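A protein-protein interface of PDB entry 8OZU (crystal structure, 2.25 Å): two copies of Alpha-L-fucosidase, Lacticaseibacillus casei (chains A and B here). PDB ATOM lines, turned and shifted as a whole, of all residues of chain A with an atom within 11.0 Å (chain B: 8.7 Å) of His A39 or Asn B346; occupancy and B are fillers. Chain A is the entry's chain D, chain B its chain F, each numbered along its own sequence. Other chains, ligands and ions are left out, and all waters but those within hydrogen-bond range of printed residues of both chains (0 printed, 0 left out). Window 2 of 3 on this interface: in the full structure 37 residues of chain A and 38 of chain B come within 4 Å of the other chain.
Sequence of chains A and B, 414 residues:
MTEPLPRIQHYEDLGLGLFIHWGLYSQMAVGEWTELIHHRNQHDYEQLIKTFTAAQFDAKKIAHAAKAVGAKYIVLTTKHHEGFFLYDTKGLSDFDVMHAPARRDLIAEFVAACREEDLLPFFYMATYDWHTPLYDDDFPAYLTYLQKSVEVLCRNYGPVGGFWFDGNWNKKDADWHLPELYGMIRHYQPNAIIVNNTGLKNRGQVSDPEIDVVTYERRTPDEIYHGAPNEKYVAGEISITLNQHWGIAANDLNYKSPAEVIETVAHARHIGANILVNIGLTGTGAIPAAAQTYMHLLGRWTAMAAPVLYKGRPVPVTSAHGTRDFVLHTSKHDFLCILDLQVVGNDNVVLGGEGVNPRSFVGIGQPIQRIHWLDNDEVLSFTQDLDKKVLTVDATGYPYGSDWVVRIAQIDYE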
ATOM      1  N   VAL A  30      18.941  -0.493   8.479  1.00  0.00           N
ATOM      2  CA  VAL A  30      18.315  -0.609   7.174  1.00  0.00           C
ATOM      3  C   VAL A  30      16.867  -1.103   7.348  1.00  0.00           C
ATOM      4  O   VAL A  30      16.383  -1.924   6.553  1.00  0.00           O
ATOM      5  CB  VAL A  30      19.169  -1.474   6.198  1.00  0.00           C
ATOM      6  CG1 VAL A  30      20.461  -0.796   5.707  1.00  0.00           C
ATOM      7  CG2 VAL A  30      19.505  -2.847   6.740  1.00  0.00           C
ATOM      8  N   GLY A  31      16.178  -0.608   8.405  1.00  0.00           N
ATOM      9  CA  GLY A  31      14.784  -0.942   8.650  1.00  0.00           C
ATOM     10  C   GLY A  31      14.546  -2.224   9.463  1.00  0.00           C
ATOM     11  O   GLY A  31      15.373  -3.153   9.477  1.00  0.00           O
ATOM     12  N   GLU A  32      13.410  -2.228  10.181  1.00  0.00           N
ATOM     13  CA  GLU A  32      13.054  -3.255  11.134  1.00  0.00           C
ATOM     14  C   GLU A  32      12.734  -4.629  10.509  1.00  0.00           C
ATOM     15  O   GLU A  32      12.890  -5.640  11.173  1.00  0.00           O
ATOM     16  CB  GLU A  32      11.926  -2.733  12.052  1.00  0.00           C
ATOM     17  CG  GLU A  32      10.558  -2.640  11.441  1.00  0.00           C
ATOM     18  CD  GLU A  32      10.283  -1.497  10.476  1.00  0.00           C
ATOM     19  OE1 GLU A  32      11.194  -0.655  10.286  1.00  0.00           O
ATOM     20  OE2 GLU A  32       9.155  -1.457   9.868  1.00  0.00           O
ATOM     21  N   TRP A  33      12.324  -4.687   9.253  1.00  0.00           N
ATOM     22  CA  TRP A  33      11.986  -5.942   8.588  1.00  0.00           C
ATOM     23  C   TRP A  33      13.209  -6.584   7.905  1.00  0.00           C
ATOM     24  O   TRP A  33      13.067  -7.483   7.042  1.00  0.00           O
ATOM     25  CB  TRP A  33      10.869  -5.734   7.528  1.00  0.00           C
ATOM     26  CG  TRP A  33       9.472  -5.704   8.071  1.00  0.00           C
ATOM     27  CD1 TRP A  33       8.927  -4.772   8.888  1.00  0.00           C
ATOM     28  CD2 TRP A  33       8.400  -6.625   7.784  1.00  0.00           C
ATOM     29  NE1 TRP A  33       7.634  -5.075   9.212  1.00  0.00           N
ATOM     30  CE2 TRP A  33       7.265  -6.186   8.509  1.00  0.00           C
ATOM     31  CE3 TRP A  33       8.278  -7.766   6.976  1.00  0.00           C
ATOM     32  CZ2 TRP A  33       6.032  -6.842   8.447  1.00  0.00           C
ATOM     33  CZ3 TRP A  33       7.071  -8.449   6.969  1.00  0.00           C
ATOM     34  CH2 TRP A  33       5.969  -8.011   7.725  1.00  0.00           C
ATOM     35  N   THR A  34      14.419  -6.087   8.205  1.00  0.00           N
ATOM     36  CA  THR A  34      15.559  -6.430   7.369  1.00  0.00           C
ATOM     37  C   THR A  34      15.790  -7.956   7.279  1.00  0.00           C
ATOM     38  O   THR A  34      16.169  -8.476   6.211  1.00  0.00           O
ATOM     39  CB  THR A  34      16.799  -5.682   7.819  1.00  0.00           C
ATOM     40  OG1 THR A  34      17.820  -6.035   6.886  1.00  0.00           O
ATOM     41  CG2 THR A  34      17.227  -6.017   9.226  1.00  0.00           C
ATOM     42  N   GLU A  35      15.600  -8.670   8.384  1.00  0.00           N
ATOM     43  CA  GLU A  35      15.922 -10.091   8.399  1.00  0.00           C
ATOM     44  C   GLU A  35      15.162 -10.828   7.295  1.00  0.00           C
ATOM     45  O   GLU A  35      15.785 -11.590   6.535  1.00  0.00           O
ATOM     46  CB  GLU A  35      15.644 -10.745   9.753  1.00  0.00           C
ATOM     47  CG  GLU A  35      16.067 -12.207   9.763  1.00  0.00           C
ATOM     48  CD  GLU A  35      15.825 -12.944  11.087  1.00  0.00           C
ATOM     49  OE1 GLU A  35      15.008 -12.492  11.949  1.00  0.00           O
ATOM     50  OE2 GLU A  35      16.476 -13.966  11.284  1.00  0.00           O
ATOM     51  N   LEU A  36      13.854 -10.566   7.165  1.00  0.00           N
ATOM     52  CA  LEU A  36      13.032 -11.184   6.131  1.00  0.00           C
ATOM     53  C   LEU A  36      13.294 -10.552   4.765  1.00  0.00           C
ATOM     54  O   LEU A  36      13.567 -11.253   3.795  1.00  0.00           O
ATOM     55  CB  LEU A  36      11.535 -11.024   6.470  1.00  0.00           C
ATOM     56  CG  LEU A  36      10.545 -11.843   5.644  1.00  0.00           C
ATOM     57  CD1 LEU A  36       9.319 -12.199   6.495  1.00  0.00           C
ATOM     58  CD2 LEU A  36       9.969 -11.158   4.412  1.00  0.00           C
ATOM     59  N   ILE A  37      13.184  -9.218   4.659  1.00  0.00           N
ATOM     60  CA  ILE A  37      13.089  -8.644   3.329  1.00  0.00           C
ATOM     61  C   ILE A  37      14.447  -8.687   2.627  1.00  0.00           C
ATOM     62  O   ILE A  37      14.480  -8.787   1.398  1.00  0.00           O
ATOM     63  CB  ILE A  37      12.519  -7.224   3.399  1.00  0.00           C
ATOM     64  CG1 ILE A  37      11.075  -7.228   3.918  1.00  0.00           C
ATOM     65  CG2 ILE A  37      12.660  -6.525   2.045  1.00  0.00           C
ATOM     66  CD1 ILE A  37      10.522  -5.817   4.099  1.00  0.00           C
ATOM     67  N   HIS A  38      15.561  -8.633   3.376  1.00  0.00           N
ATOM     68  CA  HIS A  38      16.863  -8.725   2.734  1.00  0.00           C
ATOM     69  C   HIS A  38      17.321 -10.187   2.675  1.00  0.00           C
ATOM     70  O   HIS A  38      18.480 -10.424   2.346  1.00  0.00           O
ATOM     71  CB  HIS A  38      17.915  -7.848   3.436  1.00  0.00           C
ATOM     72  CG  HIS A  38      17.680  -6.379   3.320  1.00  0.00           C
ATOM     73  ND1 HIS A  38      17.588  -5.533   4.415  1.00  0.00           N
ATOM     74  CD2 HIS A  38      17.523  -5.605   2.207  1.00  0.00           C
ATOM     75  CE1 HIS A  38      17.347  -4.303   3.968  1.00  0.00           C
ATOM     76  NE2 HIS A  38      17.326  -4.312   2.635  1.00  0.00           N
ATOM     77  N   HIS A  39      16.447 -11.160   3.013  1.00  0.00           N
ATOM     78  CA  HIS A  39      16.769 -12.572   2.861  1.00  0.00           C
ATOM     79  C   HIS A  39      18.055 -12.884   3.625  1.00  0.00           C
ATOM     80  O   HIS A  39      18.975 -13.503   3.082  1.00  0.00           O
ATOM     81  CB  HIS A  39      16.932 -12.956   1.384  1.00  0.00           C
ATOM     82  CG  HIS A  39      15.643 -12.954   0.632  1.00  0.00           C
ATOM     83  ND1 HIS A  39      15.277 -11.968  -0.265  1.00  0.00           N
ATOM     84  CD2 HIS A  39      14.627 -13.840   0.641  1.00  0.00           C
ATOM     85  CE1 HIS A  39      14.077 -12.241  -0.763  1.00  0.00           C
ATOM     86  NE2 HIS A  39      13.673 -13.387  -0.238  1.00  0.00           N
ATOM     87  N   ARG A  40      18.148 -12.403   4.867  1.00  0.00           N
ATOM     88  CA  ARG A  40      19.384 -12.582   5.602  1.00  0.00           C
ATOM     89  C   ARG A  40      19.474 -14.016   6.089  1.00  0.00           C
ATOM     90  O   ARG A  40      18.443 -14.648   6.359  1.00  0.00           O
ATOM     91  CB  ARG A  40      19.473 -11.581   6.756  1.00  0.00           C
ATOM     92  CG  ARG A  40      19.827 -10.185   6.285  1.00  0.00           C
ATOM     93  CD  ARG A  40      20.054  -9.331   7.518  1.00  0.00           C
ATOM     94  NE  ARG A  40      19.944  -7.953   7.154  1.00  0.00           N
ATOM     95  CZ  ARG A  40      20.951  -7.134   6.986  1.00  0.00           C
ATOM     96  NH1 ARG A  40      20.698  -5.926   6.519  1.00  0.00           N
ATOM     97  NH2 ARG A  40      22.182  -7.514   7.286  1.00  0.00           N
ATOM     98  N   ASN A  41      20.726 -14.483   6.210  1.00  0.00           N
ATOM     99  CA  ASN A  41      20.999 -15.732   6.896  1.00  0.00           C
ATOM    100  C   ASN A  41      20.598 -15.610   8.370  1.00  0.00           C
ATOM    101  O   ASN A  41      21.131 -14.781   9.055  1.00  0.00           O
ATOM    102  CB  ASN A  41      22.472 -16.110   6.702  1.00  0.00           C
ATOM    103  CG  ASN A  41      22.810 -17.412   7.407  1.00  0.00           C
ATOM    104  OD1 ASN A  41      23.145 -17.426   8.596  1.00  0.00           O
ATOM    105  ND2 ASN A  41      22.731 -18.523   6.694  1.00  0.00           N
ATOM    106  N   GLN A  42      19.729 -16.471   8.869  1.00  0.00           N
ATOM    107  CA  GLN A  42      19.143 -16.302  10.193  1.00  0.00           C
ATOM    108  C   GLN A  42      20.233 -16.478  11.242  1.00  0.00           C
ATOM    109  O   GLN A  42      20.276 -15.736  12.221  1.00  0.00           O
ATOM    110  CB  GLN A  42      18.024 -17.324  10.436  1.00  0.00           C
ATOM    111  CG  GLN A  42      17.443 -17.279  11.835  1.00  0.00           C
ATOM    112  CD  GLN A  42      16.207 -18.120  12.077  1.00  0.00           C
ATOM    113  OE1 GLN A  42      15.985 -19.162  11.456  1.00  0.00           O
ATOM    114  NE2 GLN A  42      15.405 -17.711  13.045  1.00  0.00           N
ATOM    115  N   HIS A  43      21.113 -17.474  11.074  1.00  0.00           N
ATOM    116  CA  HIS A  43      22.156 -17.696  12.064  1.00  0.00           C
ATOM    117  C   HIS A  43      22.988 -16.410  12.157  1.00  0.00           C
ATOM    118  O   HIS A  43      23.278 -15.969  13.244  1.00  0.00           O
ATOM    119  CB  HIS A  43      22.969 -18.970  11.789  1.00  0.00           C
ATOM    120  CG  HIS A  43      24.170 -19.114  12.671  1.00  0.00           C
ATOM    121  ND1 HIS A  43      25.376 -18.463  12.431  1.00  0.00           N
ATOM    122  CD2 HIS A  43      24.345 -19.837  13.793  1.00  0.00           C
ATOM    123  CE1 HIS A  43      26.238 -18.710  13.430  1.00  0.00           C
ATOM    124  NE2 HIS A  43      25.643 -19.567  14.244  1.00  0.00           N
ATOM    125  N   ASP A  44      23.388 -15.809  11.028  1.00  0.00           N
ATOM    126  CA  ASP A  44      24.276 -14.662  11.058  1.00  0.00           C
ATOM    127  C   ASP A  44      23.554 -13.449  11.626  1.00  0.00           C
ATOM    128  O   ASP A  44      24.164 -12.736  12.422  1.00  0.00           O
ATOM    129  CB  ASP A  44      24.918 -14.399   9.701  1.00  0.00           C
ATOM    130  CG  ASP A  44      25.852 -15.530   9.238  1.00  0.00           C
ATOM    131  OD1 ASP A  44      26.320 -16.340  10.076  1.00  0.00           O
ATOM    132  OD2 ASP A  44      26.077 -15.635   8.021  1.00  0.00           O
ATOM    133  N   TYR A  45      22.277 -13.228  11.269  1.00  0.00           N
ATOM    134  CA  TYR A  45      21.492 -12.105  11.779  1.00  0.00           C
ATOM    135  C   TYR A  45      21.367 -12.177  13.299  1.00  0.00           C
ATOM    136  O   TYR A  45      21.607 -11.195  13.995  1.00  0.00           O
ATOM    137  CB  TYR A  45      20.098 -12.059  11.139  1.00  0.00           C
ATOM    138  CG  TYR A  45      19.197 -10.968  11.659  1.00  0.00           C
ATOM    139  CD1 TYR A  45      19.287  -9.687  11.139  1.00  0.00           C
ATOM    140  CD2 TYR A  45      18.281 -11.199  12.691  1.00  0.00           C
ATOM    141  CE1 TYR A  45      18.472  -8.670  11.607  1.00  0.00           C
ATOM    142  CE2 TYR A  45      17.458 -10.195  13.157  1.00  0.00           C
ATOM    143  CZ  TYR A  45      17.558  -8.925  12.613  1.00  0.00           C
ATOM    144  OH  TYR A  45      16.790  -7.850  13.006  1.00  0.00           O
ATOM    145  N   GLU A  46      21.087 -13.372  13.820  1.00  0.00           N
ATOM    146  CA  GLU A  46      20.809 -13.546  15.237  1.00  0.00           C
ATOM    147  C   GLU A  46      22.061 -13.398  16.098  1.00  0.00           C
ATOM    148  O   GLU A  46      21.955 -13.156  17.303  1.00  0.00           O
ATOM    149  CB  GLU A  46      20.098 -14.881  15.438  1.00  0.00           C
ATOM    150  CG  GLU A  46      18.685 -14.864  14.811  1.00  0.00           C
ATOM    151  CD  GLU A  46      17.712 -15.922  15.251  1.00  0.00           C
ATOM    152  OE1 GLU A  46      18.168 -16.824  15.950  1.00  0.00           O
ATOM    153  OE2 GLU A  46      16.489 -15.814  14.947  1.00  0.00           O
ATOM    154  N   TYR A 128       3.444 -12.216  14.790  1.00  0.00           N
ATOM    155  CA  TYR A 128       4.111 -12.893  13.685  1.00  0.00           C
ATOM    156  C   TYR A 128       5.619 -12.894  14.010  1.00  0.00           C
ATOM    157  O   TYR A 128       6.212 -11.834  14.031  1.00  0.00           O
ATOM    158  CB  TYR A 128       3.763 -12.152  12.392  1.00  0.00           C
ATOM    159  CG  TYR A 128       4.451 -12.562  11.111  1.00  0.00           C
ATOM    160  CD1 TYR A 128       4.821 -13.871  10.819  1.00  0.00           C
ATOM    161  CD2 TYR A 128       4.640 -11.621  10.109  1.00  0.00           C
ATOM    162  CE1 TYR A 128       5.428 -14.198   9.617  1.00  0.00           C
ATOM    163  CE2 TYR A 128       5.216 -11.931   8.891  1.00  0.00           C
ATOM    164  CZ  TYR A 128       5.610 -13.224   8.649  1.00  0.00           C
ATOM    165  OH  TYR A 128       6.182 -13.465   7.427  1.00  0.00           O
ATOM    166  N   TRP A 130       9.573 -14.629  13.508  1.00  0.00           N
ATOM    167  CA  TRP A 130      10.476 -15.246  12.529  1.00  0.00           C
ATOM    168  C   TRP A 130      11.547 -16.105  13.227  1.00  0.00           C
ATOM    169  O   TRP A 130      12.364 -16.735  12.566  1.00  0.00           O
ATOM    170  CB  TRP A 130      11.187 -14.181  11.679  1.00  0.00           C
ATOM    171  CG  TRP A 130      10.278 -13.229  10.965  1.00  0.00           C
ATOM    172  CD1 TRP A 130       8.972 -13.441  10.612  1.00  0.00           C
ATOM    173  CD2 TRP A 130      10.592 -11.891  10.540  1.00  0.00           C
ATOM    174  NE1 TRP A 130       8.442 -12.334  10.001  1.00  0.00           N
ATOM    175  CE2 TRP A 130       9.437 -11.388   9.891  1.00  0.00           C
ATOM    176  CE3 TRP A 130      11.734 -11.074  10.642  1.00  0.00           C
ATOM    177  CZ2 TRP A 130       9.401 -10.112   9.341  1.00  0.00           C
ATOM    178  CZ3 TRP A 130      11.683  -9.808  10.102  1.00  0.00           C
ATOM    179  CH2 TRP A 130      10.533  -9.349   9.453  1.00  0.00           C
ATOM    180  N   ASN A 170      -0.918 -11.961   9.380  1.00  0.00           N
ATOM    181  CA  ASN A 170      -0.105 -12.933   8.662  1.00  0.00           C
ATOM    182  C   ASN A 170      -0.904 -14.227   8.413  1.00  0.00           C
ATOM    183  O   ASN A 170      -0.582 -14.998   7.498  1.00  0.00           O
ATOM    184  CB  ASN A 170       1.176 -13.269   9.414  1.00  0.00           C
ATOM    185  CG  ASN A 170       1.990 -14.359   8.742  1.00  0.00           C
ATOM    186  OD1 ASN A 170       2.150 -15.458   9.269  1.00  0.00           O
ATOM    187  ND2 ASN A 170       2.510 -14.072   7.566  1.00  0.00           N
ATOM    188  N   HIS A 245      10.529   4.190   7.059  1.00  0.00           N
ATOM    189  CA  HIS A 245      10.707   2.974   7.833  1.00  0.00           C
ATOM    190  C   HIS A 245      10.390   3.254   9.309  1.00  0.00           C
ATOM    191  O   HIS A 245      10.301   4.401   9.708  1.00  0.00           O
ATOM    192  CB  HIS A 245      12.149   2.504   7.650  1.00  0.00           C
ATOM    193  CG  HIS A 245      12.479   2.184   6.233  1.00  0.00           C
ATOM    194  ND1 HIS A 245      12.873   3.159   5.339  1.00  0.00           N
ATOM    195  CD2 HIS A 245      12.470   0.990   5.571  1.00  0.00           C
ATOM    196  CE1 HIS A 245      13.076   2.580   4.149  1.00  0.00           C
ATOM    197  NE2 HIS A 245      12.842   1.256   4.277  1.00  0.00           N
ATOM    198  N   VAL B 343      10.144   1.878  -2.399  1.00  0.00           N
ATOM    199  CA  VAL B 343      10.962   0.859  -1.774  1.00  0.00           C
ATOM    200  C   VAL B 343      10.555  -0.547  -2.232  1.00  0.00           C
ATOM    201  O   VAL B 343       9.361  -0.794  -2.403  1.00  0.00           O
ATOM    202  CB  VAL B 343      10.881   1.021  -0.243  1.00  0.00           C
ATOM    203  CG1 VAL B 343      11.854   0.083   0.421  1.00  0.00           C
ATOM    204  CG2 VAL B 343      11.181   2.442   0.213  1.00  0.00           C
ATOM    205  N   VAL B 344      11.531  -1.441  -2.398  1.00  0.00           N
ATOM    206  CA  VAL B 344      11.292  -2.823  -2.777  1.00  0.00           C
ATOM    207  C   VAL B 344      11.158  -3.680  -1.529  1.00  0.00           C
ATOM    208  O   VAL B 344      12.110  -3.770  -0.737  1.00  0.00           O
ATOM    209  CB  VAL B 344      12.463  -3.384  -3.624  1.00  0.00           C
ATOM    210  CG1 VAL B 344      12.261  -4.861  -3.985  1.00  0.00           C
ATOM    211  CG2 VAL B 344      12.747  -2.560  -4.868  1.00  0.00           C
ATOM    212  N   GLY B 345      10.004  -4.329  -1.390  1.00  0.00           N
ATOM    213  CA  GLY B 345       9.807  -5.364  -0.382  1.00  0.00           C
ATOM    214  C   GLY B 345      10.063  -6.753  -0.953  1.00  0.00           C
ATOM    215  O   GLY B 345      11.163  -7.029  -1.428  1.00  0.00           O
ATOM    216  N   ASN B 346       9.024  -7.595  -0.911  1.00  0.00           N
ATOM    217  CA  ASN B 346       9.050  -8.975  -1.385  1.00  0.00           C
ATOM    218  C   ASN B 346       7.747  -9.300  -2.118  1.00  0.00           C
ATOM    219  O   ASN B 346       6.850  -8.444  -2.229  1.00  0.00           O
ATOM    220  CB  ASN B 346       9.130  -9.980  -0.234  1.00  0.00           C
ATOM    221  CG  ASN B 346      10.551 -10.389   0.076  1.00  0.00           C
ATOM    222  OD1 ASN B 346      11.495 -10.151  -0.689  1.00  0.00           O
ATOM    223  ND2 ASN B 346      10.729 -10.940   1.260  1.00  0.00           N
ATOM    224  N   ASP B 347       7.661 -10.569  -2.564  1.00  0.00           N
ATOM    225  CA  ASP B 347       6.411 -11.142  -3.045  1.00  0.00           C
ATOM    226  C   ASP B 347       5.330 -10.996  -1.962  1.00  0.00           C
ATOM    227  O   ASP B 347       4.207 -10.582  -2.258  1.00  0.00           O
ATOM    228  CB  ASP B 347       6.622 -12.588  -3.528  1.00  0.00           C
ATOM    229  CG  ASP B 347       6.386 -12.807  -5.025  1.00  0.00           C
ATOM    230  OD1 ASP B 347       5.270 -12.507  -5.490  1.00  0.00           O
ATOM    231  OD2 ASP B 347       7.310 -13.284  -5.721  1.00  0.00           O
ATOM    232  N   ASN B 348       5.691 -11.290  -0.703  1.00  0.00           N
ATOM    233  CA  ASN B 348       4.712 -11.312   0.384  1.00  0.00           C
ATOM    234  C   ASN B 348       4.565  -9.954   1.058  1.00  0.00           C
ATOM    235  O   ASN B 348       3.483  -9.699   1.584  1.00  0.00           O
ATOM    236  CB  ASN B 348       4.973 -12.441   1.393  1.00  0.00           C
ATOM    237  CG  ASN B 348       3.969 -13.564   1.185  1.00  0.00           C
ATOM    238  OD1 ASN B 348       3.648 -13.879   0.043  1.00  0.00           O
ATOM    239  ND2 ASN B 348       3.339 -14.045   2.245  1.00  0.00           N
ATOM    240  N   VAL B 349       5.622  -9.117   1.076  1.00  0.00           N
ATOM    241  CA  VAL B 349       5.491  -7.793   1.675  1.00  0.00           C
ATOM    242  C   VAL B 349       5.614  -6.753   0.565  1.00  0.00           C
ATOM    243  O   VAL B 349       6.719  -6.525   0.069  1.00  0.00           O
ATOM    244  CB  VAL B 349       6.550  -7.527   2.776  1.00  0.00           C
ATOM    245  CG1 VAL B 349       6.158  -6.321   3.654  1.00  0.00           C
ATOM    246  CG2 VAL B 349       6.833  -8.789   3.595  1.00  0.00           C
ATOM    247  N   VAL B 350       4.508  -6.097   0.220  1.00  0.00           N
ATOM    248  CA  VAL B 350       4.486  -5.206  -0.928  1.00  0.00           C
ATOM    249  C   VAL B 350       4.612  -3.770  -0.417  1.00  0.00           C
ATOM    250  O   VAL B 350       3.801  -3.301   0.399  1.00  0.00           O
ATOM    251  CB  VAL B 350       3.189  -5.414  -1.745  1.00  0.00           C
ATOM    252  CG1 VAL B 350       3.020  -4.466  -2.944  1.00  0.00           C
ATOM    253  CG2 VAL B 350       3.087  -6.864  -2.206  1.00  0.00           C
ATOM    254  N   LEU B 351       5.641  -3.077  -0.907  1.00  0.00           N
ATOM    255  CA  LEU B 351       5.888  -1.696  -0.520  1.00  0.00           C
ATOM    256  C   LEU B 351       5.723  -0.734  -1.697  1.00  0.00           C
ATOM    257  O   LEU B 351       5.689   0.476  -1.478  1.00  0.00           O
ATOM    258  CB  LEU B 351       7.313  -1.626   0.060  1.00  0.00           C
ATOM    259  CG  LEU B 351       7.524  -2.443   1.324  1.00  0.00           C
ATOM    260  CD1 LEU B 351       8.989  -2.449   1.714  1.00  0.00           C
ATOM    261  CD2 LEU B 351       6.657  -1.907   2.475  1.00  0.00           C
ATOM    262  N   GLY B 352       5.679  -1.240  -2.941  1.00  0.00           N
ATOM    263  CA  GLY B 352       5.357  -0.425  -4.103  1.00  0.00           C
ATOM    264  C   GLY B 352       6.445  -0.471  -5.184  1.00  0.00           C
ATOM    265  O   GLY B 352       6.162  -0.199  -6.337  1.00  0.00           O
ATOM    266  N   GLY B 353       7.692  -0.816  -4.851  1.00  0.00           N
ATOM    267  CA  GLY B 353       8.778  -0.713  -5.811  1.00  0.00           C
ATOM    268  C   GLY B 353       9.206  -2.062  -6.404  1.00  0.00           C
ATOM    269  O   GLY B 353      10.271  -2.153  -7.063  1.00  0.00           O
ATOM    270  N   GLU B 354       8.374  -3.128  -6.255  1.00  0.00           N
ATOM    271  CA  GLU B 354       8.856  -4.446  -6.635  1.00  0.00           C
ATOM    272  C   GLU B 354       8.652  -4.689  -8.119  1.00  0.00           C
ATOM    273  O   GLU B 354       9.469  -5.427  -8.682  1.00  0.00           O
ATOM    274  CB  GLU B 354       8.435  -5.610  -5.724  1.00  0.00           C
ATOM    275  CG  GLU B 354       7.096  -5.479  -5.022  1.00  0.00           C
ATOM    276  CD  GLU B 354       6.911  -4.409  -3.971  1.00  0.00           C
ATOM    277  OE1 GLU B 354       6.049  -3.543  -4.169  1.00  0.00           O
ATOM    278  OE2 GLU B 354       7.591  -4.471  -2.929  1.00  0.00           O
ATOM    279  N   GLY B 355       7.678  -4.049  -8.795  1.00  0.00           N
ATOM    280  CA  GLY B 355       7.500  -4.329 -10.224  1.00  0.00           C
ATOM    281  C   GLY B 355       8.601  -3.704 -11.100  1.00  0.00           C
ATOM    282  O   GLY B 355       9.200  -2.712 -10.705  1.00  0.00           O
ATOM    283  N   TYR B 400      15.160  -2.083   0.620  1.00  0.00           N
ATOM    284  CA  TYR B 400      14.442  -1.848   1.856  1.00  0.00           C
ATOM    285  C   TYR B 400      15.430  -1.225   2.825  1.00  0.00           C
ATOM    286  O   TYR B 400      16.600  -1.635   2.841  1.00  0.00           O
ATOM    287  CB  TYR B 400      13.890  -3.150   2.435  1.00  0.00           C
ATOM    288  CG  TYR B 400      13.236  -2.990   3.780  1.00  0.00           C
ATOM    289  CD1 TYR B 400      12.004  -2.388   3.876  1.00  0.00           C
ATOM    290  CD2 TYR B 400      13.898  -3.283   4.962  1.00  0.00           C
ATOM    291  CE1 TYR B 400      11.333  -2.273   5.098  1.00  0.00           C
ATOM    292  CE2 TYR B 400      13.306  -3.059   6.190  1.00  0.00           C
ATOM    293  CZ  TYR B 400      12.003  -2.588   6.275  1.00  0.00           C
ATOM    294  OH  TYR B 400      11.445  -2.408   7.530  1.00  0.00           O
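N of Trp A33 lies within hydrogen-bond range of OH of Tyr B400 (3.0 Å). The side-chain carboxylate (OE1) of Glu A32 is in hydrogen-bond range of the side-chain hydroxyl (OH) of Tyr B400 (3.3 Å). NE2 of His A38 sits at hydrogen-bond distance from O of Tyr B400 (2.8 Å).
OG1 of Thr A34 lies within hydrogen-bond range of NE of Arg A40, 2.9 Å away. The side-chain carboxylate (OE2) of Glu B354 is in hydrogen-bond range of the backbone NH (N) of Gly B345 (2.9 Å). A ring nitrogen (ND1) of His A38 lies within hydrogen-bond range of the side-chain hydroxyl (OG1) of Thr A34 (2.5 Å).
O of Val A30 touches CD2 of Tyr B400 (3.2 Å). Gly A31 touches Tyr B400. Trp A33 touches Val B349 (CZ3 to CG2, 3.4 Å). Thr A34 touches Tyr B400. Asn B346 touches Leu A36. CG2 of Ile A37 touches O of Val B344, 3.95 Å away. O of Gly B345 touches CG2 of Ile A37, 3.8 Å away. Asn B346 touches Ile A37. Asn B346 touches His A39. CE1 of Tyr B400 touches CD2 of His A245, at 3.5 Å.
Of chain B, only Asn B346 (3.3 Å) comes within 4 Å of His A39. Asn B346 touches three residues of chain A. Asp B347 touches none of the printed residues of chain A. Val B350 touches none of the printed residues of chain A. Printed residues of chain B within 4 Å of Trp A33: Val B349 (3.4 Å) and Tyr B400 (3.0 Å). Printed residues of chain A within 4 Å of Val B344: Ile A37 (3.95 Å). Of the printed residues of chain A, Tyr B400 touches Val A30 (3.2 Å), Gly A31 (3.6 Å), Glu A32 (3.3 Å), Trp A33 (3.0 Å), Thr A34 (3.8 Å), Ile A37 (3.6 Å), His A38 (2.8 Å) and His A245 (3.5 Å). Of the printed residues of chain A, Val B349 touches Trp A33 (3.4 Å). Tyr A128 touches none of the printed residues of chain B. Asp A44 touches none of the printed residues of chain B. The nearest residue of chain B that does not touch His A39 is Gly B345 (6.0 Å). The nearest printed residue of chain B that does not touch Thr A34 is Asn B346 (7.8 Å).
Printed residues of chain A that touch a printed residue of chain B: Val A30, Gly A31, Glu A32, Trp A33, Thr A34, Leu A36, Ile A37, His A38, His A39 and His A245. Hydrophobic or aromatic side chains of chain A that line the printed part of chain B: Trp A33, Leu A36, Ile A37, His A38, His A39 and His A245. Of the 14 printed residues of chain B, 5 touch a printed residue of chain A. Hydrophobic or aromatic side chains of chain B within 4 Å of the printed part of chain A: Val B349 and Tyr B400.
No position is printed for both chains. Of the 14 pairs that touch across the chains among the printed residues, none has its exchanged pair printed and touching as well.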
